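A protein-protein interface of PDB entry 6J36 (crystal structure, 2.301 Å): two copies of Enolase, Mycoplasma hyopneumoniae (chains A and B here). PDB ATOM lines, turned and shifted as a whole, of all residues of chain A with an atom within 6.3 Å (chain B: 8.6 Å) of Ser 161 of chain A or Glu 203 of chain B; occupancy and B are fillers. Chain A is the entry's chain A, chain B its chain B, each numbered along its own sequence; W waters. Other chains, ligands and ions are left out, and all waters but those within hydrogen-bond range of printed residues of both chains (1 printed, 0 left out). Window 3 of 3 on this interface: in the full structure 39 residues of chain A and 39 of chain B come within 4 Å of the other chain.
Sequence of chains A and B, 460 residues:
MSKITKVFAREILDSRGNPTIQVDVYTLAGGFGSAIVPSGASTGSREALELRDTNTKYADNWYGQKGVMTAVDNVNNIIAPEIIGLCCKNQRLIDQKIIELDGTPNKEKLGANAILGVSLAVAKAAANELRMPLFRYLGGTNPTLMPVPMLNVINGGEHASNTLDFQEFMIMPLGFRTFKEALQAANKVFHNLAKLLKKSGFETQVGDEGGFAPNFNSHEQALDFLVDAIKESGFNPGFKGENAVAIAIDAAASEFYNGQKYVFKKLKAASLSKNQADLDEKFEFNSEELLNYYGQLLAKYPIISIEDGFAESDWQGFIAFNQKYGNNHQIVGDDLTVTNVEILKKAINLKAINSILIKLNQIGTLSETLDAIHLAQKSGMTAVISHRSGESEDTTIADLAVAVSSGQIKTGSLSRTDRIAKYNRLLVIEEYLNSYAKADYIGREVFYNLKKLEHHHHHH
Water W1 lies within hydrogen-bond range of O of Gln 205 of chain A (2.6 Å), NE2 of Gln 205 of chain B (2.9 Å), O of Glu 203 of chain A (3.1 Å) and N of Ala 213 of chain A (3.1 Å).
OE2 of Glu 203 of chain A sits at hydrogen-bond distance from OG of Ser 161 of chain B (3.1 Å). N of Ala 213 of chain A lies within hydrogen-bond range of OE1 of Gln 205 of chain B, 3.5 Å away. OE1 of Gln 205 of chain A is in hydrogen-bond range of N of Ala 213 of chain B, 3.3 Å away. The side-chain hydroxyl (OG) of Ser 161 of chain A lies within hydrogen-bond range of the side-chain carboxylate (OE2) of Glu 203 of chain B (2.5 Å). O of Gln 205 of chain A sits close to OE1 of Gln 205 of chain B (3.2 Å).
Hydrophobic or aromatic side chains of chain A within 4 Å of the printed part of chain B: Ala 213. Of the 22 printed residues of chain B, 6 touch a printed residue of chain A. Among the printed residues, 7 pairs touch across the chains. Among the printed residues, no Asp or Glu carboxylate lies within 4 Å of a Lys or Arg side-chain nitrogen of the other chain.
Of chain B, only Lys 198 (3.98 Å) and Glu 203 (2.5 Å) come within 4 Å of Ser 161 of chain A. Of chain A, only Ser 161 (2.5 Å) comes within 4 Å of Glu 203 of chain B. Printed residues of chain A within 4 Å of Ala 213 of chain B: Gln 205 (3.3 Å). Of the printed residues of chain B, Gln 205 of chain A touches Gln 205, Val 206 and Ala 213. Of the printed residues of chain A, Lys 198 of chain B touches Ser 161 (3.98 Å). Of the printed residues of chain A, Val 206 of chain B touches Gln 205 (3.3 Å). Phe 202 of chain B touches none of the printed residues of chain A. Gly 201 of chain B touches none of the printed residues of chain A. The nearest residue of chain B that does not touch Ser 161 of chain A is Phe 202 of chain B (5.7 Å). The nearest residue of chain A that does not touch Glu 203 of chain B is Gln 205 of chain A (4.8 Å).
Among the printed residues, pairs that only touch across the chains: Gln 205 of chain A with Val 206 of chain B and Ser 161 of chain A with Lys 198 of chain B.
Ser 161 of chain A touches Glu 203 of chain B, and with the chains exchanged Glu 203 of chain A touches Ser 161 of chain B. Gln 205 of chain A touches its own counterpart, Gln 205 of chain B. Gln 205 of chain A touches Ala 213 of chain B, and with the chains exchanged Ala 213 of chain A touches Gln 205 of chain B. Positions printed for both chains: 161, 203, 205, 213, 214 and 215.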
ATOM      1  N   GLY A 157     -15.402 -11.342 -20.652  1.00  0.00           N
ATOM      2  CA  GLY A 157     -16.490 -12.285 -20.845  1.00  0.00           C
ATOM      3  C   GLY A 157     -17.732 -11.665 -21.471  1.00  0.00           C
ATOM      4  O   GLY A 157     -17.703 -10.575 -22.050  1.00  0.00           O
ATOM      5  N   GLU A 158     -18.854 -12.367 -21.290  1.00  0.00           N
ATOM      6  CA  GLU A 158     -20.018 -12.190 -22.164  1.00  0.00           C
ATOM      7  C   GLU A 158     -20.490 -10.732 -22.221  1.00  0.00           C
ATOM      8  O   GLU A 158     -20.654 -10.163 -23.310  1.00  0.00           O
ATOM      9  CB  GLU A 158     -21.153 -13.117 -21.706  1.00  0.00           C
ATOM     10  N   HIS A 159     -20.702 -10.104 -21.061  1.00  0.00           N
ATOM     11  CA  HIS A 159     -21.421  -8.834 -21.016  1.00  0.00           C
ATOM     12  C   HIS A 159     -20.521  -7.605 -21.098  1.00  0.00           C
ATOM     13  O   HIS A 159     -21.042  -6.489 -21.212  1.00  0.00           O
ATOM     14  CB  HIS A 159     -22.275  -8.769 -19.745  1.00  0.00           C
ATOM     15  CG  HIS A 159     -23.032 -10.035 -19.471  1.00  0.00           C
ATOM     16  ND1 HIS A 159     -23.877 -10.612 -20.398  1.00  0.00           N
ATOM     17  CD2 HIS A 159     -23.055 -10.845 -18.385  1.00  0.00           C
ATOM     18  CE1 HIS A 159     -24.394 -11.717 -19.890  1.00  0.00           C
ATOM     19  NE2 HIS A 159     -23.912 -11.881 -18.670  1.00  0.00           N
ATOM     20  N   ALA A 160     -19.200  -7.774 -21.053  1.00  0.00           N
ATOM     21  CA  ALA A 160     -18.283  -6.649 -21.174  1.00  0.00           C
ATOM     22  C   ALA A 160     -18.036  -6.332 -22.645  1.00  0.00           C
ATOM     23  O   ALA A 160     -17.736  -7.226 -23.438  1.00  0.00           O
ATOM     24  CB  ALA A 160     -16.962  -6.954 -20.459  1.00  0.00           C
ATOM     25  N   SER A 161     -18.152  -5.052 -23.006  1.00  0.00           N
ATOM     26  CA  SER A 161     -17.944  -4.601 -24.380  1.00  0.00           C
ATOM     27  C   SER A 161     -16.524  -4.835 -24.901  1.00  0.00           C
ATOM     28  O   SER A 161     -16.294  -4.663 -26.105  1.00  0.00           O
ATOM     29  CB  SER A 161     -18.274  -3.106 -24.491  1.00  0.00           C
ATOM     30  OG  SER A 161     -19.514  -2.800 -23.870  1.00  0.00           O
ATOM     31  N   ASN A 162     -15.573  -5.221 -24.051  1.00  0.00           N
ATOM     32  CA  ASN A 162     -14.176  -5.298 -24.466  1.00  0.00           C
ATOM     33  C   ASN A 162     -13.902  -6.615 -25.195  1.00  0.00           C
ATOM     34  O   ASN A 162     -14.807  -7.392 -25.493  1.00  0.00           O
ATOM     35  CB  ASN A 162     -13.252  -5.118 -23.264  1.00  0.00           C
ATOM     36  CG  ASN A 162     -13.526  -6.119 -22.154  1.00  0.00           C
ATOM     37  OD1 ASN A 162     -13.880  -7.275 -22.400  1.00  0.00           O
ATOM     38  ND2 ASN A 162     -13.360  -5.674 -20.917  1.00  0.00           N
ATOM     39  N   THR A 163     -12.626  -6.877 -25.479  1.00  0.00           N
ATOM     40  CA  THR A 163     -12.197  -8.021 -26.273  1.00  0.00           C
ATOM     41  C   THR A 163     -11.577  -9.114 -25.411  1.00  0.00           C
ATOM     42  O   THR A 163     -10.828  -9.957 -25.918  1.00  0.00           O
ATOM     43  CB  THR A 163     -11.215  -7.567 -27.355  1.00  0.00           C
ATOM     44  OG1 THR A 163     -11.587  -6.268 -27.821  1.00  0.00           O
ATOM     45  CG2 THR A 163     -11.237  -8.504 -28.533  1.00  0.00           C
ATOM     46  N   GLU A 203     -12.121   3.663 -19.523  1.00  0.00           N
ATOM     47  CA  GLU A 203     -13.249   3.942 -18.654  1.00  0.00           C
ATOM     48  C   GLU A 203     -13.008   3.380 -17.263  1.00  0.00           C
ATOM     49  O   GLU A 203     -12.351   2.352 -17.080  1.00  0.00           O
ATOM     50  CB  GLU A 203     -14.535   3.361 -19.230  1.00  0.00           C
ATOM     51  CG  GLU A 203     -15.116   4.199 -20.352  1.00  0.00           C
ATOM     52  CD  GLU A 203     -15.323   5.633 -19.925  1.00  0.00           C
ATOM     53  OE1 GLU A 203     -16.140   5.851 -19.005  1.00  0.00           O
ATOM     54  OE2 GLU A 203     -14.658   6.533 -20.488  1.00  0.00           O
ATOM     55  N   GLN A 205     -15.756   3.345 -14.791  1.00  0.00           N
ATOM     56  CA  GLN A 205     -16.952   2.859 -14.121  1.00  0.00           C
ATOM     57  C   GLN A 205     -16.783   1.384 -13.755  1.00  0.00           C
ATOM     58  O   GLN A 205     -15.873   0.703 -14.227  1.00  0.00           O
ATOM     59  CB  GLN A 205     -18.172   3.054 -15.004  1.00  0.00           C
ATOM     60  CG  GLN A 205     -18.479   4.512 -15.309  1.00  0.00           C
ATOM     61  CD  GLN A 205     -19.789   4.650 -16.058  1.00  0.00           C
ATOM     62  OE1 GLN A 205     -20.844   4.916 -15.455  1.00  0.00           O
ATOM     63  NE2 GLN A 205     -19.743   4.429 -17.381  1.00  0.00           N
ATOM     64  N   ALA A 213     -13.985  -2.804 -16.252  1.00  0.00           N
ATOM     65  CA  ALA A 213     -14.084  -3.500 -17.542  1.00  0.00           C
ATOM     66  C   ALA A 213     -13.630  -2.560 -18.645  1.00  0.00           C
ATOM     67  O   ALA A 213     -14.429  -2.138 -19.482  1.00  0.00           O
ATOM     68  CB  ALA A 213     -15.507  -3.994 -17.819  1.00  0.00           C
ATOM     69  N   PRO A 214     -12.356  -2.180 -18.657  1.00  0.00           N
ATOM     70  CA  PRO A 214     -11.882  -1.240 -19.676  1.00  0.00           C
ATOM     71  C   PRO A 214     -11.815  -1.906 -21.041  1.00  0.00           C
ATOM     72  O   PRO A 214     -11.889  -3.125 -21.171  1.00  0.00           O
ATOM     73  CB  PRO A 214     -10.493  -0.826 -19.173  1.00  0.00           C
ATOM     74  CG  PRO A 214     -10.056  -1.928 -18.308  1.00  0.00           C
ATOM     75  CD  PRO A 214     -11.292  -2.541 -17.704  1.00  0.00           C
ATOM     76  N   ASN A 215     -11.670  -1.075 -22.075  1.00  0.00           N
ATOM     77  CA  ASN A 215     -11.677  -1.541 -23.462  1.00  0.00           C
ATOM     78  C   ASN A 215     -10.307  -2.098 -23.871  1.00  0.00           C
ATOM     79  O   ASN A 215      -9.646  -1.613 -24.785  1.00  0.00           O
ATOM     80  CB  ASN A 215     -12.113  -0.405 -24.382  1.00  0.00           C
ATOM     81  CG  ASN A 215     -12.672  -0.902 -25.710  1.00  0.00           C
ATOM     82  OD1 ASN A 215     -13.183  -2.025 -25.815  1.00  0.00           O
ATOM     83  ND2 ASN A 215     -12.571  -0.065 -26.736  1.00  0.00           N
ATOM     84  N   LYS A 266     -15.018 -13.142 -28.781  1.00  0.00           N
ATOM     85  CA  LYS A 266     -14.891 -11.685 -28.837  1.00  0.00           C
ATOM     86  C   LYS A 266     -13.602 -11.279 -29.532  1.00  0.00           C
ATOM     87  O   LYS A 266     -13.578 -10.313 -30.308  1.00  0.00           O
ATOM     88  CB  LYS A 266     -14.951 -11.085 -27.438  1.00  0.00           C
ATOM     89  CG  LYS A 266     -16.319 -11.171 -26.803  1.00  0.00           C
ATOM     90  CD  LYS A 266     -16.195 -11.074 -25.306  1.00  0.00           C
ATOM     91  CE  LYS A 266     -16.531  -9.688 -24.851  1.00  0.00           C
ATOM     92  NZ  LYS A 266     -15.668  -9.249 -23.714  1.00  0.00           N
ATOM     93  N   VAL B 153     -30.011   8.340 -12.139  1.00  0.00           N
ATOM     94  CA  VAL B 153     -30.026   7.348 -13.218  1.00  0.00           C
ATOM     95  C   VAL B 153     -28.950   7.656 -14.263  1.00  0.00           C
ATOM     96  O   VAL B 153     -28.343   6.732 -14.820  1.00  0.00           O
ATOM     97  CB  VAL B 153     -31.416   7.239 -13.885  1.00  0.00           C
ATOM     98  CG1 VAL B 153     -32.388   6.447 -13.017  1.00  0.00           C
ATOM     99  CG2 VAL B 153     -31.981   8.599 -14.200  1.00  0.00           C
ATOM    100  N   ILE B 154     -28.693   8.947 -14.528  1.00  0.00           N
ATOM    101  CA  ILE B 154     -27.797   9.375 -15.601  1.00  0.00           C
ATOM    102  C   ILE B 154     -26.833  10.414 -15.050  1.00  0.00           C
ATOM    103  O   ILE B 154     -27.259  11.366 -14.387  1.00  0.00           O
ATOM    104  CB  ILE B 154     -28.558   9.978 -16.799  1.00  0.00           C
ATOM    105  CG1 ILE B 154     -29.603   9.005 -17.350  1.00  0.00           C
ATOM    106  CG2 ILE B 154     -27.566  10.422 -17.862  1.00  0.00           C
ATOM    107  CD1 ILE B 154     -29.001   7.837 -18.014  1.00  0.00           C
ATOM    108  N   SER B 161     -17.018  10.694 -19.110  1.00  0.00           N
ATOM    109  CA  SER B 161     -16.475  10.881 -20.450  1.00  0.00           C
ATOM    110  C   SER B 161     -17.523  11.260 -21.502  1.00  0.00           C
ATOM    111  O   SER B 161     -17.151  11.459 -22.664  1.00  0.00           O
ATOM    112  CB  SER B 161     -15.742   9.614 -20.892  1.00  0.00           C
ATOM    113  OG  SER B 161     -16.653   8.672 -21.436  1.00  0.00           O
ATOM    114  N   LEU B 193     -34.540   1.288 -18.301  1.00  0.00           N
ATOM    115  CA  LEU B 193     -33.506   2.213 -18.760  1.00  0.00           C
ATOM    116  C   LEU B 193     -32.257   1.452 -19.187  1.00  0.00           C
ATOM    117  O   LEU B 193     -31.741   1.665 -20.284  1.00  0.00           O
ATOM    118  CB  LEU B 193     -33.169   3.241 -17.670  1.00  0.00           C
ATOM    119  CG  LEU B 193     -32.074   4.263 -18.020  1.00  0.00           C
ATOM    120  CD1 LEU B 193     -32.422   5.054 -19.291  1.00  0.00           C
ATOM    121  CD2 LEU B 193     -31.824   5.226 -16.874  1.00  0.00           C
ATOM    122  N   ALA B 194     -31.780   0.526 -18.343  1.00  0.00           N
ATOM    123  CA  ALA B 194     -30.604  -0.266 -18.697  1.00  0.00           C
ATOM    124  C   ALA B 194     -30.834  -1.069 -19.975  1.00  0.00           C
ATOM    125  O   ALA B 194     -29.952  -1.141 -20.839  1.00  0.00           O
ATOM    126  CB  ALA B 194     -30.212  -1.197 -17.547  1.00  0.00           C
ATOM    127  N   LEU B 196     -32.817  -0.357 -22.511  1.00  0.00           N
ATOM    128  CA  LEU B 196     -32.795   0.534 -23.669  1.00  0.00           C
ATOM    129  C   LEU B 196     -31.380   0.980 -24.001  1.00  0.00           C
ATOM    130  O   LEU B 196     -31.008   1.047 -25.178  1.00  0.00           O
ATOM    131  CB  LEU B 196     -33.696   1.740 -23.422  1.00  0.00           C
ATOM    132  CG  LEU B 196     -35.164   1.300 -23.297  1.00  0.00           C
ATOM    133  CD1 LEU B 196     -36.051   2.403 -22.741  1.00  0.00           C
ATOM    134  CD2 LEU B 196     -35.699   0.800 -24.635  1.00  0.00           C
ATOM    135  N   LEU B 197     -30.573   1.276 -22.976  1.00  0.00           N
ATOM    136  CA  LEU B 197     -29.194   1.703 -23.205  1.00  0.00           C
ATOM    137  C   LEU B 197     -28.386   0.607 -23.882  1.00  0.00           C
ATOM    138  O   LEU B 197     -27.592   0.880 -24.793  1.00  0.00           O
ATOM    139  CB  LEU B 197     -28.536   2.100 -21.883  1.00  0.00           C
ATOM    140  CG  LEU B 197     -29.049   3.337 -21.167  1.00  0.00           C
ATOM    141  CD1 LEU B 197     -28.557   3.317 -19.729  1.00  0.00           C
ATOM    142  CD2 LEU B 197     -28.609   4.619 -21.891  1.00  0.00           C
ATOM    143  N   LYS B 198     -28.562  -0.640 -23.440  1.00  0.00           N
ATOM    144  CA  LYS B 198     -27.900  -1.747 -24.115  1.00  0.00           C
ATOM    145  C   LYS B 198     -28.394  -1.881 -25.549  1.00  0.00           C
ATOM    146  O   LYS B 198     -27.602  -2.129 -26.464  1.00  0.00           O
ATOM    147  CB  LYS B 198     -28.123  -3.048 -23.343  1.00  0.00           C
ATOM    148  CG  LYS B 198     -27.176  -3.251 -22.170  1.00  0.00           C
ATOM    149  CD  LYS B 198     -25.811  -3.787 -22.620  1.00  0.00           C
ATOM    150  CE  LYS B 198     -24.669  -2.801 -22.305  1.00  0.00           C
ATOM    151  NZ  LYS B 198     -23.365  -3.193 -22.945  1.00  0.00           N
ATOM    152  N   LYS B 199     -29.697  -1.689 -25.771  1.00  0.00           N
ATOM    153  CA  LYS B 199     -30.246  -1.823 -27.119  1.00  0.00           C
ATOM    154  C   LYS B 199     -29.649  -0.802 -28.081  1.00  0.00           C
ATOM    155  O   LYS B 199     -29.521  -1.081 -29.279  1.00  0.00           O
ATOM    156  CB  LYS B 199     -31.769  -1.687 -27.093  1.00  0.00           C
ATOM    157  CG  LYS B 199     -32.539  -3.001 -26.984  1.00  0.00           C
ATOM    158  CD  LYS B 199     -33.989  -2.736 -26.535  1.00  0.00           C
ATOM    159  CE  LYS B 199     -34.821  -4.018 -26.434  1.00  0.00           C
ATOM    160  NZ  LYS B 199     -34.159  -5.078 -25.617  1.00  0.00           N
ATOM    161  N   SER B 200     -29.282   0.380 -27.589  1.00  0.00           N
ATOM    162  CA  SER B 200     -28.693   1.409 -28.433  1.00  0.00           C
ATOM    163  C   SER B 200     -27.178   1.432 -28.357  1.00  0.00           C
ATOM    164  O   SER B 200     -26.557   2.387 -28.821  1.00  0.00           O
ATOM    165  CB  SER B 200     -29.255   2.779 -28.070  1.00  0.00           C
ATOM    166  OG  SER B 200     -30.614   2.875 -28.464  1.00  0.00           O
ATOM    167  N   GLY B 201     -26.568   0.415 -27.767  1.00  0.00           N
ATOM    168  CA  GLY B 201     -25.127   0.331 -27.789  1.00  0.00           C
ATOM    169  C   GLY B 201     -24.390   1.186 -26.785  1.00  0.00           C
ATOM    170  O   GLY B 201     -23.197   1.419 -26.971  1.00  0.00           O
ATOM    171  N   PHE B 202     -25.046   1.647 -25.718  1.00  0.00           N
ATOM    172  CA  PHE B 202     -24.375   2.422 -24.683  1.00  0.00           C
ATOM    173  C   PHE B 202     -23.846   1.511 -23.581  1.00  0.00           C
ATOM    174  O   PHE B 202     -24.251   0.356 -23.441  1.00  0.00           O
ATOM    175  CB  PHE B 202     -25.315   3.471 -24.077  1.00  0.00           C
ATOM    176  CG  PHE B 202     -25.726   4.553 -25.044  1.00  0.00           C
ATOM    177  CD1 PHE B 202     -24.816   5.524 -25.448  1.00  0.00           C
ATOM    178  CD2 PHE B 202     -27.024   4.594 -25.552  1.00  0.00           C
ATOM    179  CE1 PHE B 202     -25.192   6.514 -26.345  1.00  0.00           C
ATOM    180  CE2 PHE B 202     -27.414   5.592 -26.451  1.00  0.00           C
ATOM    181  CZ  PHE B 202     -26.495   6.544 -26.855  1.00  0.00           C
ATOM    182  N   GLU B 203     -22.922   2.050 -22.796  1.00  0.00           N
ATOM    183  CA  GLU B 203     -22.367   1.309 -21.678  1.00  0.00           C
ATOM    184  C   GLU B 203     -23.316   1.335 -20.488  1.00  0.00           C
ATOM    185  O   GLU B 203     -24.026   2.316 -20.235  1.00  0.00           O
ATOM    186  CB  GLU B 203     -21.010   1.876 -21.260  1.00  0.00           C
ATOM    187  CG  GLU B 203     -19.836   1.452 -22.162  1.00  0.00           C
ATOM    188  CD  GLU B 203     -19.839  -0.034 -22.499  1.00  0.00           C
ATOM    189  OE1 GLU B 203     -19.752  -0.856 -21.557  1.00  0.00           O
ATOM    190  OE2 GLU B 203     -19.929  -0.380 -23.702  1.00  0.00           O
ATOM    191  N   THR B 204     -23.293   0.249 -19.734  1.00  0.00           N
ATOM    192  CA  THR B 204     -24.207   0.077 -18.626  1.00  0.00           C
ATOM    193  C   THR B 204     -23.488  -0.137 -17.295  1.00  0.00           C
ATOM    194  O   THR B 204     -24.135  -0.438 -16.287  1.00  0.00           O
ATOM    195  CB  THR B 204     -25.157  -1.072 -18.975  1.00  0.00           C
ATOM    196  OG1 THR B 204     -26.373  -0.906 -18.249  1.00  0.00           O
ATOM    197  CG2 THR B 204     -24.522  -2.430 -18.696  1.00  0.00           C
ATOM    198  N   GLN B 205     -22.169   0.039 -17.260  1.00  0.00           N
ATOM    199  CA  GLN B 205     -21.440   0.117 -16.007  1.00  0.00           C
ATOM    200  C   GLN B 205     -21.899   1.334 -15.198  1.00  0.00           C
ATOM    201  O   GLN B 205     -22.531   2.250 -15.718  1.00  0.00           O
ATOM    202  CB  GLN B 205     -19.950   0.199 -16.289  1.00  0.00           C
ATOM    203  CG  GLN B 205     -19.325  -1.060 -16.859  1.00  0.00           C
ATOM    204  CD  GLN B 205     -17.802  -1.014 -16.683  1.00  0.00           C
ATOM    205  OE1 GLN B 205     -17.241  -1.675 -15.789  1.00  0.00           O
ATOM    206  NE2 GLN B 205     -17.129  -0.192 -17.509  1.00  0.00           N
ATOM    207  N   VAL B 206     -21.572   1.345 -13.903  1.00  0.00           N
ATOM    208  CA  VAL B 206     -22.110   2.364 -13.005  1.00  0.00           C
ATOM    209  C   VAL B 206     -20.987   3.139 -12.315  1.00  0.00           C
ATOM    210  O   VAL B 206     -19.846   2.682 -12.213  1.00  0.00           O
ATOM    211  CB  VAL B 206     -23.068   1.754 -11.959  1.00  0.00           C
ATOM    212  CG1 VAL B 206     -24.144   0.933 -12.659  1.00  0.00           C
ATOM    213  CG2 VAL B 206     -22.294   0.896 -10.956  1.00  0.00           C
ATOM    214  N   GLY B 211     -25.620   4.698 -10.606  1.00  0.00           N
ATOM    215  CA  GLY B 211     -26.285   5.087 -11.827  1.00  0.00           C
ATOM    216  C   GLY B 211     -25.361   4.953 -13.031  1.00  0.00           C
ATOM    217  O   GLY B 211     -24.222   4.514 -12.924  1.00  0.00           O
ATOM    218  N   PHE B 212     -25.881   5.352 -14.193  1.00  0.00           N
ATOM    219  CA  PHE B 212     -25.206   5.184 -15.472  1.00  0.00           C
ATOM    220  C   PHE B 212     -24.583   6.491 -15.942  1.00  0.00           C
ATOM    221  O   PHE B 212     -25.045   7.586 -15.608  1.00  0.00           O
ATOM    222  CB  PHE B 212     -26.190   4.676 -16.544  1.00  0.00           C
ATOM    223  CG  PHE B 212     -26.971   3.483 -16.119  1.00  0.00           C
ATOM    224  CD1 PHE B 212     -26.338   2.270 -15.901  1.00  0.00           C
ATOM    225  CD2 PHE B 212     -28.333   3.569 -15.899  1.00  0.00           C
ATOM    226  CE1 PHE B 212     -27.047   1.168 -15.485  1.00  0.00           C
ATOM    227  CE2 PHE B 212     -29.050   2.462 -15.481  1.00  0.00           C
ATOM    228  CZ  PHE B 212     -28.411   1.260 -15.283  1.00  0.00           C
ATOM    229  N   ALA B 213     -23.526   6.368 -16.737  1.00  0.00           N
ATOM    230  CA  ALA B 213     -22.936   7.507 -17.447  1.00  0.00           C
ATOM    231  C   ALA B 213     -22.688   7.099 -18.890  1.00  0.00           C
ATOM    232  O   ALA B 213     -21.541   6.930 -19.313  1.00  0.00           O
ATOM    233  CB  ALA B 213     -21.646   7.984 -16.779  1.00  0.00           C
ATOM    234  N   PRO B 214     -23.745   6.931 -19.676  1.00  0.00           N
ATOM    235  CA  PRO B 214     -23.573   6.538 -21.077  1.00  0.00           C
ATOM    236  C   PRO B 214     -23.130   7.733 -21.913  1.00  0.00           C
ATOM    237  O   PRO B 214     -23.190   8.880 -21.474  1.00  0.00           O
ATOM    238  CB  PRO B 214     -24.963   6.038 -21.480  1.00  0.00           C
ATOM    239  CG  PRO B 214     -25.909   6.765 -20.571  1.00  0.00           C
ATOM    240  CD  PRO B 214     -25.159   7.145 -19.315  1.00  0.00           C
ATOM    241  N   ASN B 215     -22.671   7.440 -23.135  1.00  0.00           N
ATOM    242  CA  ASN B 215     -22.057   8.439 -24.017  1.00  0.00           C
ATOM    243  C   ASN B 215     -23.097   9.291 -24.763  1.00  0.00           C
ATOM    244  O   ASN B 215     -23.137   9.350 -25.990  1.00  0.00           O
ATOM    245  CB  ASN B 215     -21.120   7.742 -24.996  1.00  0.00           C
ATOM    246  CG  ASN B 215     -20.087   8.690 -25.603  1.00  0.00           C
ATOM    247  OD1 ASN B 215     -19.881   9.812 -25.123  1.00  0.00           O
ATOM    248  ND2 ASN B 215     -19.430   8.236 -26.665  1.00  0.00           N
ATOM    249  N   PHE B 216     -23.944   9.982 -24.002  1.00  0.00           N
ATOM    250  CA  PHE B 216     -24.896  10.909 -24.606  1.00  0.00           C
ATOM    251  C   PHE B 216     -24.177  12.148 -25.139  1.00  0.00           C
ATOM    252  O   PHE B 216     -23.156  12.583 -24.597  1.00  0.00           O
ATOM    253  CB  PHE B 216     -25.958  11.335 -23.593  1.00  0.00           C
ATOM    254  CG  PHE B 216     -26.965  10.263 -23.264  1.00  0.00           C
ATOM    255  CD1 PHE B 216     -27.566   9.518 -24.265  1.00  0.00           C
ATOM    256  CD2 PHE B 216     -27.321  10.014 -21.949  1.00  0.00           C
ATOM    257  CE1 PHE B 216     -28.498   8.543 -23.959  1.00  0.00           C
ATOM    258  CE2 PHE B 216     -28.253   9.040 -21.638  1.00  0.00           C
ATOM    259  CZ  PHE B 216     -28.842   8.306 -22.644  1.00  0.00           C
HETATM  260  O   HOH W   1     -14.519   0.290 -16.441  1.00  0.00           O
